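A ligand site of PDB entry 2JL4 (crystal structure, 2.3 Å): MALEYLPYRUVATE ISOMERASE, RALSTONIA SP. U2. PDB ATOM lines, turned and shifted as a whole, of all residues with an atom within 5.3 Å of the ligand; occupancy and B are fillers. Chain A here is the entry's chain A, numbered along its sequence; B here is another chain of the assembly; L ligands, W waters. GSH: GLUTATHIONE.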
ATOM      1  N   SER A  10      19.170  34.284  10.694  1.00  0.00           N
ATOM      2  CA  SER A  10      18.927  32.943  11.243  1.00  0.00           C
ATOM      3  C   SER A  10      19.931  31.920  10.696  1.00  0.00           C
ATOM      4  O   SER A  10      20.055  31.736   9.471  1.00  0.00           O
ATOM      5  CB  SER A  10      17.494  32.510  10.950  1.00  0.00           C
ATOM      6  OG  SER A  10      17.330  31.106  11.171  1.00  0.00           O
ATOM      7  N   GLY A  11      20.641  31.256  11.607  1.00  0.00           N
ATOM      8  CA  GLY A  11      21.638  30.242  11.248  1.00  0.00           C
ATOM      9  C   GLY A  11      21.062  29.016  10.529  1.00  0.00           C
ATOM     10  O   GLY A  11      21.653  28.528   9.554  1.00  0.00           O
ATOM     11  N   THR A  12      19.919  28.535  11.015  1.00  0.00           N
ATOM     12  CA  THR A  12      19.200  27.432  10.375  1.00  0.00           C
ATOM     13  C   THR A  12      18.629  27.851   9.008  1.00  0.00           C
ATOM     14  O   THR A  12      18.680  27.070   8.064  1.00  0.00           O
ATOM     15  CB  THR A  12      18.071  26.887  11.285  1.00  0.00           C
ATOM     16  OG1 THR A  12      17.179  27.957  11.643  1.00  0.00           O
ATOM     17  CG2 THR A  12      18.650  26.255  12.580  1.00  0.00           C
ATOM     18  N   SER A  13      18.084  29.064   8.903  1.00  0.00           N
ATOM     19  CA  SER A  13      17.661  29.609   7.603  1.00  0.00           C
ATOM     20  C   SER A  13      18.810  29.599   6.587  1.00  0.00           C
ATOM     21  O   SER A  13      18.651  29.157   5.436  1.00  0.00           O
ATOM     22  CB  SER A  13      17.151  31.048   7.752  1.00  0.00           C
ATOM     23  OG  SER A  13      16.009  31.130   8.567  1.00  0.00           O
ATOM     24  N   ARG A  15      21.556  27.815   6.775  1.00  0.00           N
ATOM     25  CA  ARG A  15      21.841  26.409   6.514  1.00  0.00           C
ATOM     26  C   ARG A  15      20.984  25.868   5.351  1.00  0.00           C
ATOM     27  O   ARG A  15      21.501  25.267   4.408  1.00  0.00           O
ATOM     28  CB  ARG A  15      21.607  25.615   7.792  1.00  0.00           C
ATOM     29  CG  ARG A  15      21.932  24.122   7.740  1.00  0.00           C
ATOM     30  CD  ARG A  15      21.348  23.416   8.959  1.00  0.00           C
ATOM     31  NE  ARG A  15      21.821  23.965  10.233  1.00  0.00           N
ATOM     32  CZ  ARG A  15      21.261  23.740  11.423  1.00  0.00           C
ATOM     33  NH1 ARG A  15      20.173  22.965  11.537  1.00  0.00           N
ATOM     34  NH2 ARG A  15      21.805  24.277  12.508  1.00  0.00           N
ATOM     35  N   LEU A  34      12.272  37.748  13.069  1.00  0.00           N
ATOM     36  CA  LEU A  34      12.411  37.234  14.441  1.00  0.00           C
ATOM     37  C   LEU A  34      12.511  38.356  15.485  1.00  0.00           C
ATOM     38  O   LEU A  34      11.993  38.224  16.583  1.00  0.00           O
ATOM     39  CB  LEU A  34      13.600  36.275  14.564  1.00  0.00           C
ATOM     40  CG  LEU A  34      13.681  35.083  13.591  1.00  0.00           C
ATOM     41  CD1 LEU A  34      14.949  34.295  13.840  1.00  0.00           C
ATOM     42  CD2 LEU A  34      12.458  34.178  13.678  1.00  0.00           C
ATOM     43  N   HIS A  39       7.272  35.363  14.205  1.00  0.00           N
ATOM     44  CA  HIS A  39       7.178  33.915  14.417  1.00  0.00           C
ATOM     45  C   HIS A  39       6.374  33.528  15.665  1.00  0.00           C
ATOM     46  O   HIS A  39       5.892  32.387  15.774  1.00  0.00           O
ATOM     47  CB  HIS A  39       8.581  33.302  14.476  1.00  0.00           C
ATOM     48  CG  HIS A  39       9.395  33.768  15.651  1.00  0.00           C
ATOM     49  ND1 HIS A  39       9.746  35.076  15.842  1.00  0.00           N
ATOM     50  CD2 HIS A  39       9.922  33.075  16.689  1.00  0.00           C
ATOM     51  CE1 HIS A  39      10.455  35.188  16.962  1.00  0.00           C
ATOM     52  NE2 HIS A  39      10.586  33.986  17.488  1.00  0.00           N
ATOM     53  N   LEU A  40       6.205  34.455  16.602  1.00  0.00           N
ATOM     54  CA  LEU A  40       5.486  34.157  17.850  1.00  0.00           C
ATOM     55  C   LEU A  40       3.999  34.471  17.742  1.00  0.00           C
ATOM     56  O   LEU A  40       3.239  34.284  18.709  1.00  0.00           O
ATOM     57  CB  LEU A  40       6.105  34.866  19.047  1.00  0.00           C
ATOM     58  CG  LEU A  40       7.512  34.418  19.436  1.00  0.00           C
ATOM     59  CD1 LEU A  40       7.921  35.072  20.759  1.00  0.00           C
ATOM     60  CD2 LEU A  40       7.615  32.881  19.514  1.00  0.00           C
ATOM     61  N   GLN A  51       6.730  27.169  15.736  1.00  0.00           N
ATOM     62  CA  GLN A  51       6.992  28.617  15.692  1.00  0.00           C
ATOM     63  C   GLN A  51       8.475  28.938  15.710  1.00  0.00           C
ATOM     64  O   GLN A  51       8.958  29.758  16.506  1.00  0.00           O
ATOM     65  CB  GLN A  51       6.215  29.380  16.793  1.00  0.00           C
ATOM     66  CG  GLN A  51       4.716  29.450  16.549  1.00  0.00           C
ATOM     67  CD  GLN A  51       3.952  30.095  17.680  1.00  0.00           C
ATOM     68  OE1 GLN A  51       3.745  29.491  18.726  1.00  0.00           O
ATOM     69  NE2 GLN A  51       3.504  31.319  17.469  1.00  0.00           N
ATOM     70  N   LEU A  52       9.211  28.244  14.839  1.00  0.00           N
ATOM     71  CA  LEU A  52      10.619  28.571  14.562  1.00  0.00           C
ATOM     72  C   LEU A  52      10.830  28.661  13.043  1.00  0.00           C
ATOM     73  O   LEU A  52      10.019  28.162  12.269  1.00  0.00           O
ATOM     74  CB  LEU A  52      11.559  27.534  15.179  1.00  0.00           C
ATOM     75  CG  LEU A  52      11.614  27.289  16.701  1.00  0.00           C
ATOM     76  CD1 LEU A  52      12.500  26.053  17.057  1.00  0.00           C
ATOM     77  CD2 LEU A  52      12.056  28.524  17.486  1.00  0.00           C
ATOM     78  N   VAL A  53      11.897  29.317  12.616  1.00  0.00           N
ATOM     79  CA  VAL A  53      12.273  29.275  11.217  1.00  0.00           C
ATOM     80  C   VAL A  53      13.456  28.304  11.054  1.00  0.00           C
ATOM     81  O   VAL A  53      14.188  28.061  11.996  1.00  0.00           O
ATOM     82  CB  VAL A  53      12.577  30.670  10.620  1.00  0.00           C
ATOM     83  CG1 VAL A  53      11.307  31.548  10.607  1.00  0.00           C
ATOM     84  CG2 VAL A  53      13.739  31.367  11.325  1.00  0.00           C
ATOM     85  N   PRO A  54      13.626  27.741   9.848  1.00  0.00           N
ATOM     86  CA  PRO A  54      12.826  27.956   8.649  1.00  0.00           C
ATOM     87  C   PRO A  54      11.645  26.988   8.514  1.00  0.00           C
ATOM     88  O   PRO A  54      11.588  25.980   9.218  1.00  0.00           O
ATOM     89  CB  PRO A  54      13.835  27.703   7.531  1.00  0.00           C
ATOM     90  CG  PRO A  54      14.752  26.623   8.106  1.00  0.00           C
ATOM     91  CD  PRO A  54      14.731  26.796   9.605  1.00  0.00           C
ATOM     92  N   ILE A  64       8.884  21.402   8.134  1.00  0.00           N
ATOM     93  CA  ILE A  64       9.634  22.019   9.229  1.00  0.00           C
ATOM     94  C   ILE A  64      10.828  21.141   9.608  1.00  0.00           C
ATOM     95  O   ILE A  64      10.915  19.986   9.158  1.00  0.00           O
ATOM     96  CB  ILE A  64       8.720  22.310  10.465  1.00  0.00           C
ATOM     97  CG1 ILE A  64       8.201  20.992  11.068  1.00  0.00           C
ATOM     98  CG2 ILE A  64       7.561  23.255  10.068  1.00  0.00           C
ATOM     99  CD1 ILE A  64       7.875  21.071  12.574  1.00  0.00           C
ATOM    100  N   GLN A  65      11.744  21.715  10.405  1.00  0.00           N
ATOM    101  CA  GLN A  65      13.003  21.075  10.831  1.00  0.00           C
ATOM    102  C   GLN A  65      14.054  20.986   9.731  1.00  0.00           C
ATOM    103  O   GLN A  65      14.041  20.060   8.910  1.00  0.00           O
ATOM    104  CB  GLN A  65      12.782  19.709  11.490  1.00  0.00           C
ATOM    105  CG  GLN A  65      12.166  19.779  12.882  1.00  0.00           C
ATOM    106  CD  GLN A  65      13.034  20.494  13.903  1.00  0.00           C
ATOM    107  OE1 GLN A  65      14.271  20.423  13.857  1.00  0.00           O
ATOM    108  NE2 GLN A  65      12.402  21.170  14.832  1.00  0.00           N
ATOM    109  N   SER A  66      14.983  21.947   9.736  1.00  0.00           N
ATOM    110  CA  SER A  66      16.009  22.041   8.696  1.00  0.00           C
ATOM    111  C   SER A  66      16.840  20.763   8.497  1.00  0.00           C
ATOM    112  O   SER A  66      17.141  20.434   7.350  1.00  0.00           O
ATOM    113  CB  SER A  66      16.893  23.305   8.872  1.00  0.00           C
ATOM    114  OG  SER A  66      17.862  23.155   9.876  1.00  0.00           O
ATOM    115  N   PRO A  67      17.196  20.033   9.578  1.00  0.00           N
ATOM    116  CA  PRO A  67      17.932  18.777   9.356  1.00  0.00           C
ATOM    117  C   PRO A  67      17.139  17.776   8.510  1.00  0.00           C
ATOM    118  O   PRO A  67      17.717  17.150   7.622  1.00  0.00           O
ATOM    119  CB  PRO A  67      18.103  18.219  10.774  1.00  0.00           C
ATOM    120  CG  PRO A  67      18.053  19.408  11.658  1.00  0.00           C
ATOM    121  CD  PRO A  67      16.998  20.275  11.021  1.00  0.00           C
ATOM    122  N   HIS A 105      24.279  25.216  17.702  1.00  0.00           N
ATOM    123  CA  HIS A 105      23.267  26.184  17.326  1.00  0.00           C
ATOM    124  C   HIS A 105      22.127  26.348  18.347  1.00  0.00           C
ATOM    125  O   HIS A 105      21.790  27.477  18.707  1.00  0.00           O
ATOM    126  CB  HIS A 105      22.664  25.910  15.943  1.00  0.00           C
ATOM    127  CG  HIS A 105      21.357  26.604  15.747  1.00  0.00           C
ATOM    128  ND1 HIS A 105      20.149  26.040  16.111  1.00  0.00           N
ATOM    129  CD2 HIS A 105      21.070  27.859  15.319  1.00  0.00           C
ATOM    130  CE1 HIS A 105      19.176  26.901  15.884  1.00  0.00           C
ATOM    131  NE2 HIS A 105      19.708  28.016  15.406  1.00  0.00           N
ATOM    132  N   ASN A 109      20.330  30.041  20.462  1.00  0.00           N
ATOM    133  CA  ASN A 109      19.091  30.509  19.838  1.00  0.00           C
ATOM    134  C   ASN A 109      18.488  31.684  20.606  1.00  0.00           C
ATOM    135  O   ASN A 109      18.653  31.805  21.836  1.00  0.00           O
ATOM    136  CB  ASN A 109      18.089  29.351  19.792  1.00  0.00           C
ATOM    137  CG  ASN A 109      17.052  29.490  18.673  1.00  0.00           C
ATOM    138  OD1 ASN A 109      17.168  30.359  17.793  1.00  0.00           O
ATOM    139  ND2 ASN A 109      16.040  28.616  18.706  1.00  0.00           N
ATOM    140  N   ARG A 110      17.796  32.559  19.871  1.00  0.00           N
ATOM    141  CA  ARG A 110      17.161  33.774  20.415  1.00  0.00           C
ATOM    142  C   ARG A 110      16.362  33.562  21.714  1.00  0.00           C
ATOM    143  O   ARG A 110      16.502  34.324  22.686  1.00  0.00           O
ATOM    144  CB  ARG A 110      16.250  34.414  19.358  1.00  0.00           C
ATOM    145  CG  ARG A 110      15.744  35.800  19.729  1.00  0.00           C
ATOM    146  CD  ARG A 110      14.648  36.266  18.787  1.00  0.00           C
ATOM    147  NE  ARG A 110      14.222  37.629  19.119  1.00  0.00           N
ATOM    148  CZ  ARG A 110      13.298  37.928  20.027  1.00  0.00           C
ATOM    149  NH1 ARG A 110      12.688  36.960  20.701  1.00  0.00           N
ATOM    150  NH2 ARG A 110      12.988  39.187  20.267  1.00  0.00           N
ATOM    151  N   ARG A 111      15.513  32.528  21.711  1.00  0.00           N
ATOM    152  CA  ARG A 111      14.622  32.245  22.831  1.00  0.00           C
ATOM    153  C   ARG A 111      15.413  31.960  24.099  1.00  0.00           C
ATOM    154  O   ARG A 111      15.023  32.377  25.182  1.00  0.00           O
ATOM    155  CB  ARG A 111      13.675  31.080  22.489  1.00  0.00           C
ATOM    156  CG  ARG A 111      14.398  29.741  22.270  1.00  0.00           C
ATOM    157  CD  ARG A 111      13.555  28.697  21.566  1.00  0.00           C
ATOM    158  NE  ARG A 111      14.279  27.433  21.545  1.00  0.00           N
ATOM    159  CZ  ARG A 111      13.776  26.250  21.869  1.00  0.00           C
ATOM    160  NH1 ARG A 111      12.486  26.119  22.198  1.00  0.00           N
ATOM    161  NH2 ARG A 111      14.568  25.183  21.825  1.00  0.00           N
ATOM    162  N   ILE A 112      16.537  31.261  23.939  1.00  0.00           N
ATOM    163  CA  ILE A 112      17.429  30.902  25.041  1.00  0.00           C
ATOM    164  C   ILE A 112      18.095  32.140  25.626  1.00  0.00           C
ATOM    165  O   ILE A 112      18.133  32.342  26.840  1.00  0.00           O
ATOM    166  CB  ILE A 112      18.552  29.892  24.604  1.00  0.00           C
ATOM    167  CG1 ILE A 112      17.994  28.671  23.829  1.00  0.00           C
ATOM    168  CG2 ILE A 112      19.426  29.474  25.794  1.00  0.00           C
ATOM    169  CD1 ILE A 112      16.903  27.857  24.529  1.00  0.00           C
ATOM    170  N   ALA B  98      13.980  15.433  15.276  1.00  0.00           N
ATOM    171  CA  ALA B  98      14.802  16.621  15.388  1.00  0.00           C
ATOM    172  C   ALA B  98      14.237  17.667  16.362  1.00  0.00           C
ATOM    173  O   ALA B  98      14.975  18.499  16.884  1.00  0.00           O
ATOM    174  CB  ALA B  98      15.051  17.241  13.980  1.00  0.00           C
ATOM    175  N   CYS B 102      17.361  18.258  18.542  1.00  0.00           N
ATOM    176  CA  CYS B 102      17.930  19.599  18.368  1.00  0.00           C
ATOM    177  C   CYS B 102      17.364  20.595  19.382  1.00  0.00           C
ATOM    178  O   CYS B 102      18.120  21.378  19.968  1.00  0.00           O
ATOM    179  CB  CYS B 102      17.653  20.115  16.953  1.00  0.00           C
ATOM    180  SG  CYS B 102      18.468  19.196  15.615  1.00  0.00           S
ATOM    181  N   ASP B 103      16.040  20.550  19.566  1.00  0.00           N
ATOM    182  CA  ASP B 103      15.308  21.640  20.206  1.00  0.00           C
ATOM    183  C   ASP B 103      14.902  21.413  21.670  1.00  0.00           C
ATOM    184  O   ASP B 103      14.463  22.350  22.335  1.00  0.00           O
ATOM    185  CB  ASP B 103      14.088  22.030  19.335  1.00  0.00           C
ATOM    186  CG  ASP B 103      14.484  22.376  17.892  1.00  0.00           C
ATOM    187  OD1 ASP B 103      15.657  22.744  17.638  1.00  0.00           O
ATOM    188  OD2 ASP B 103      13.612  22.304  16.996  1.00  0.00           O
HETATM  189  N1  GSH L   1      15.890  22.382  14.757  1.00  0.00           N
HETATM  190  CA1 GSH L   1      15.283  23.564  14.166  1.00  0.00           C
HETATM  191  C1  GSH L   1      15.612  23.604  12.691  1.00  0.00           C
HETATM  192  O11 GSH L   1      16.781  23.385  12.371  1.00  0.00           O
HETATM  193  O12 GSH L   1      14.708  23.851  11.862  1.00  0.00           O
HETATM  194  CB1 GSH L   1      15.808  24.811  14.871  1.00  0.00           C
HETATM  195  CG1 GSH L   1      15.109  26.061  14.348  1.00  0.00           C
HETATM  196  CD1 GSH L   1      15.463  27.291  15.156  1.00  0.00           C
HETATM  197  OE1 GSH L   1      15.791  27.181  16.329  1.00  0.00           O
HETATM  198  N2  GSH L   1      15.382  28.455  14.503  1.00  0.00           N
HETATM  199  CA2 GSH L   1      15.677  29.738  15.118  1.00  0.00           C
HETATM  200  C2  GSH L   1      14.428  30.480  15.536  1.00  0.00           C
HETATM  201  O2  GSH L   1      13.407  30.429  14.866  1.00  0.00           O
HETATM  202  CB2 GSH L   1      16.464  30.607  14.138  1.00  0.00           C
HETATM  203  SG2 GSH L   1      18.165  30.029  13.863  1.00  0.00           S
HETATM  204  N3  GSH L   1      14.488  31.185  16.649  1.00  0.00           N
HETATM  205  CA3 GSH L   1      13.350  31.938  17.140  1.00  0.00           C
HETATM  206  C3  GSH L   1      13.365  32.044  18.638  1.00  0.00           C
HETATM  207  O31 GSH L   1      14.327  31.553  19.276  1.00  0.00           O
HETATM  208  O32 GSH L   1      12.409  32.618  19.197  1.00  0.00           O
HETATM  209  O   HOH W   1      18.561  22.045  13.933  1.00  0.00           O
HETATM  210  O   HOH W   2      12.528  34.315  21.243  1.00  0.00           O
HETATM  211  O   HOH W   3      16.691  25.460  18.212  1.00  0.00           O
HETATM  212  O   HOH W   4      12.160  24.378  11.324  1.00  0.00           O
HETATM  213  O   HOH W   5      10.721  30.891  20.667  1.00  0.00           O
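The side-chain amide oxygen of Gln 65 sits at hydrogen-bond distance from a nitrogen (N1) of the ligand, at 2.7 Å. An oxygen (O12) of the ligand lies within hydrogen-bond range of the backbone NH of Ser 66, 2.9 Å away. An oxygen (O11) of the ligand lies within hydrogen-bond range of the side-chain hydroxyl (OG) of Ser 66, 2.7 Å away. ND2 of Asn 109 sits at hydrogen-bond distance from OE1 of the ligand. An oxygen (O2) of the ligand lies within hydrogen-bond range of the backbone NH of Val 53, at 2.9 Å. O of Val 53 lies within hydrogen-bond range of N2 of the ligand. NE2 of His 39 sits at hydrogen-bond distance from O32 of the ligand (2.8 Å). N of Arg 111 is in hydrogen-bond range of O31 of the ligand, at 2.9 Å. A nitrogen (N1) of the ligand is in salt-bridge range of the side-chain carboxylate (OD1) of Asp 103 of chain B (2.9 Å). SG2 of the ligand lies close to NE2 of His 105 (3.0 Å). OG of Ser 10 sits close to SG2 of the ligand (3.0 Å). SG2 of the ligand lies close to N of Thr 12 (3.7 Å). SG2 of the ligand sits close to OG1 of Thr 12 (3.2 Å). The guanidinium group (NH1) of Arg 15 is in salt-bridge range of an oxygen (O11) of the ligand (3.5 Å). The backbone NH of Gly 11 lies close to a sulfur (SG2) of the ligand, 3.6 Å away.
OD2 of Asp 103 of chain B is in hydrogen-bond range of NE2 of Gln 65 (2.7 Å). NH1 of Arg 15 is in hydrogen-bond range of OG of Ser 66, 2.9 Å away. O of Val 53 is in hydrogen-bond range of OG1 of Thr 12. O of His 39 sits at hydrogen-bond distance from NE2 of Gln 51 (3.1 Å). The backbone carbonyl oxygen (O) of Asp 103 of chain B sits at hydrogen-bond distance from the guanidinium group (NH2) of Arg 111 (2.9 Å). The side-chain hydroxyl (OG) of Ser 13 is in hydrogen-bond range of the side-chain hydroxyl (OG) of Ser 10 (2.9 Å). NE of Arg 110 is in hydrogen-bond range of O of Leu 34 (3.4 Å). O of Ala 98 of chain B lies close to SG of Cys 102 of chain B.
Leu 34 touches the ligand. Leu 52 touches the ligand (CA to O2, 3.4 Å). CD of Pro 54 touches O12 of the ligand (3.7 Å). Pro 67 touches the ligand (CD to O11, 3.4 Å). Arg 110 touches the ligand (CB to O31, 3.4 Å). Cys 102 of chain B touches the ligand. Hydrophobic or aromatic side chains within 4 Å of the ligand: Leu 34, His 39, Leu 52, Val 53, Pro 54, Pro 67 and His 105. Of the 24 residues printed, 18 come within 4 Å of the ligand.
Water W4 lies within hydrogen-bond range of O12 of the ligand, O of Pro 54 and N of Gln 65. Water W2 lies within hydrogen-bond range of an oxygen (O32) of the ligand and the guanidinium group of Arg 110. Water W3 lies within hydrogen-bond range of OE1 of the ligand, OD1 of Asp 103 of chain B and ND2 of Asn 109. Water W1 lies within hydrogen-bond range of O11 of the ligand (2.7 Å), NH1 of Arg 15 (3.0 Å) and SG of Cys 102 of chain B (3.3 Å).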
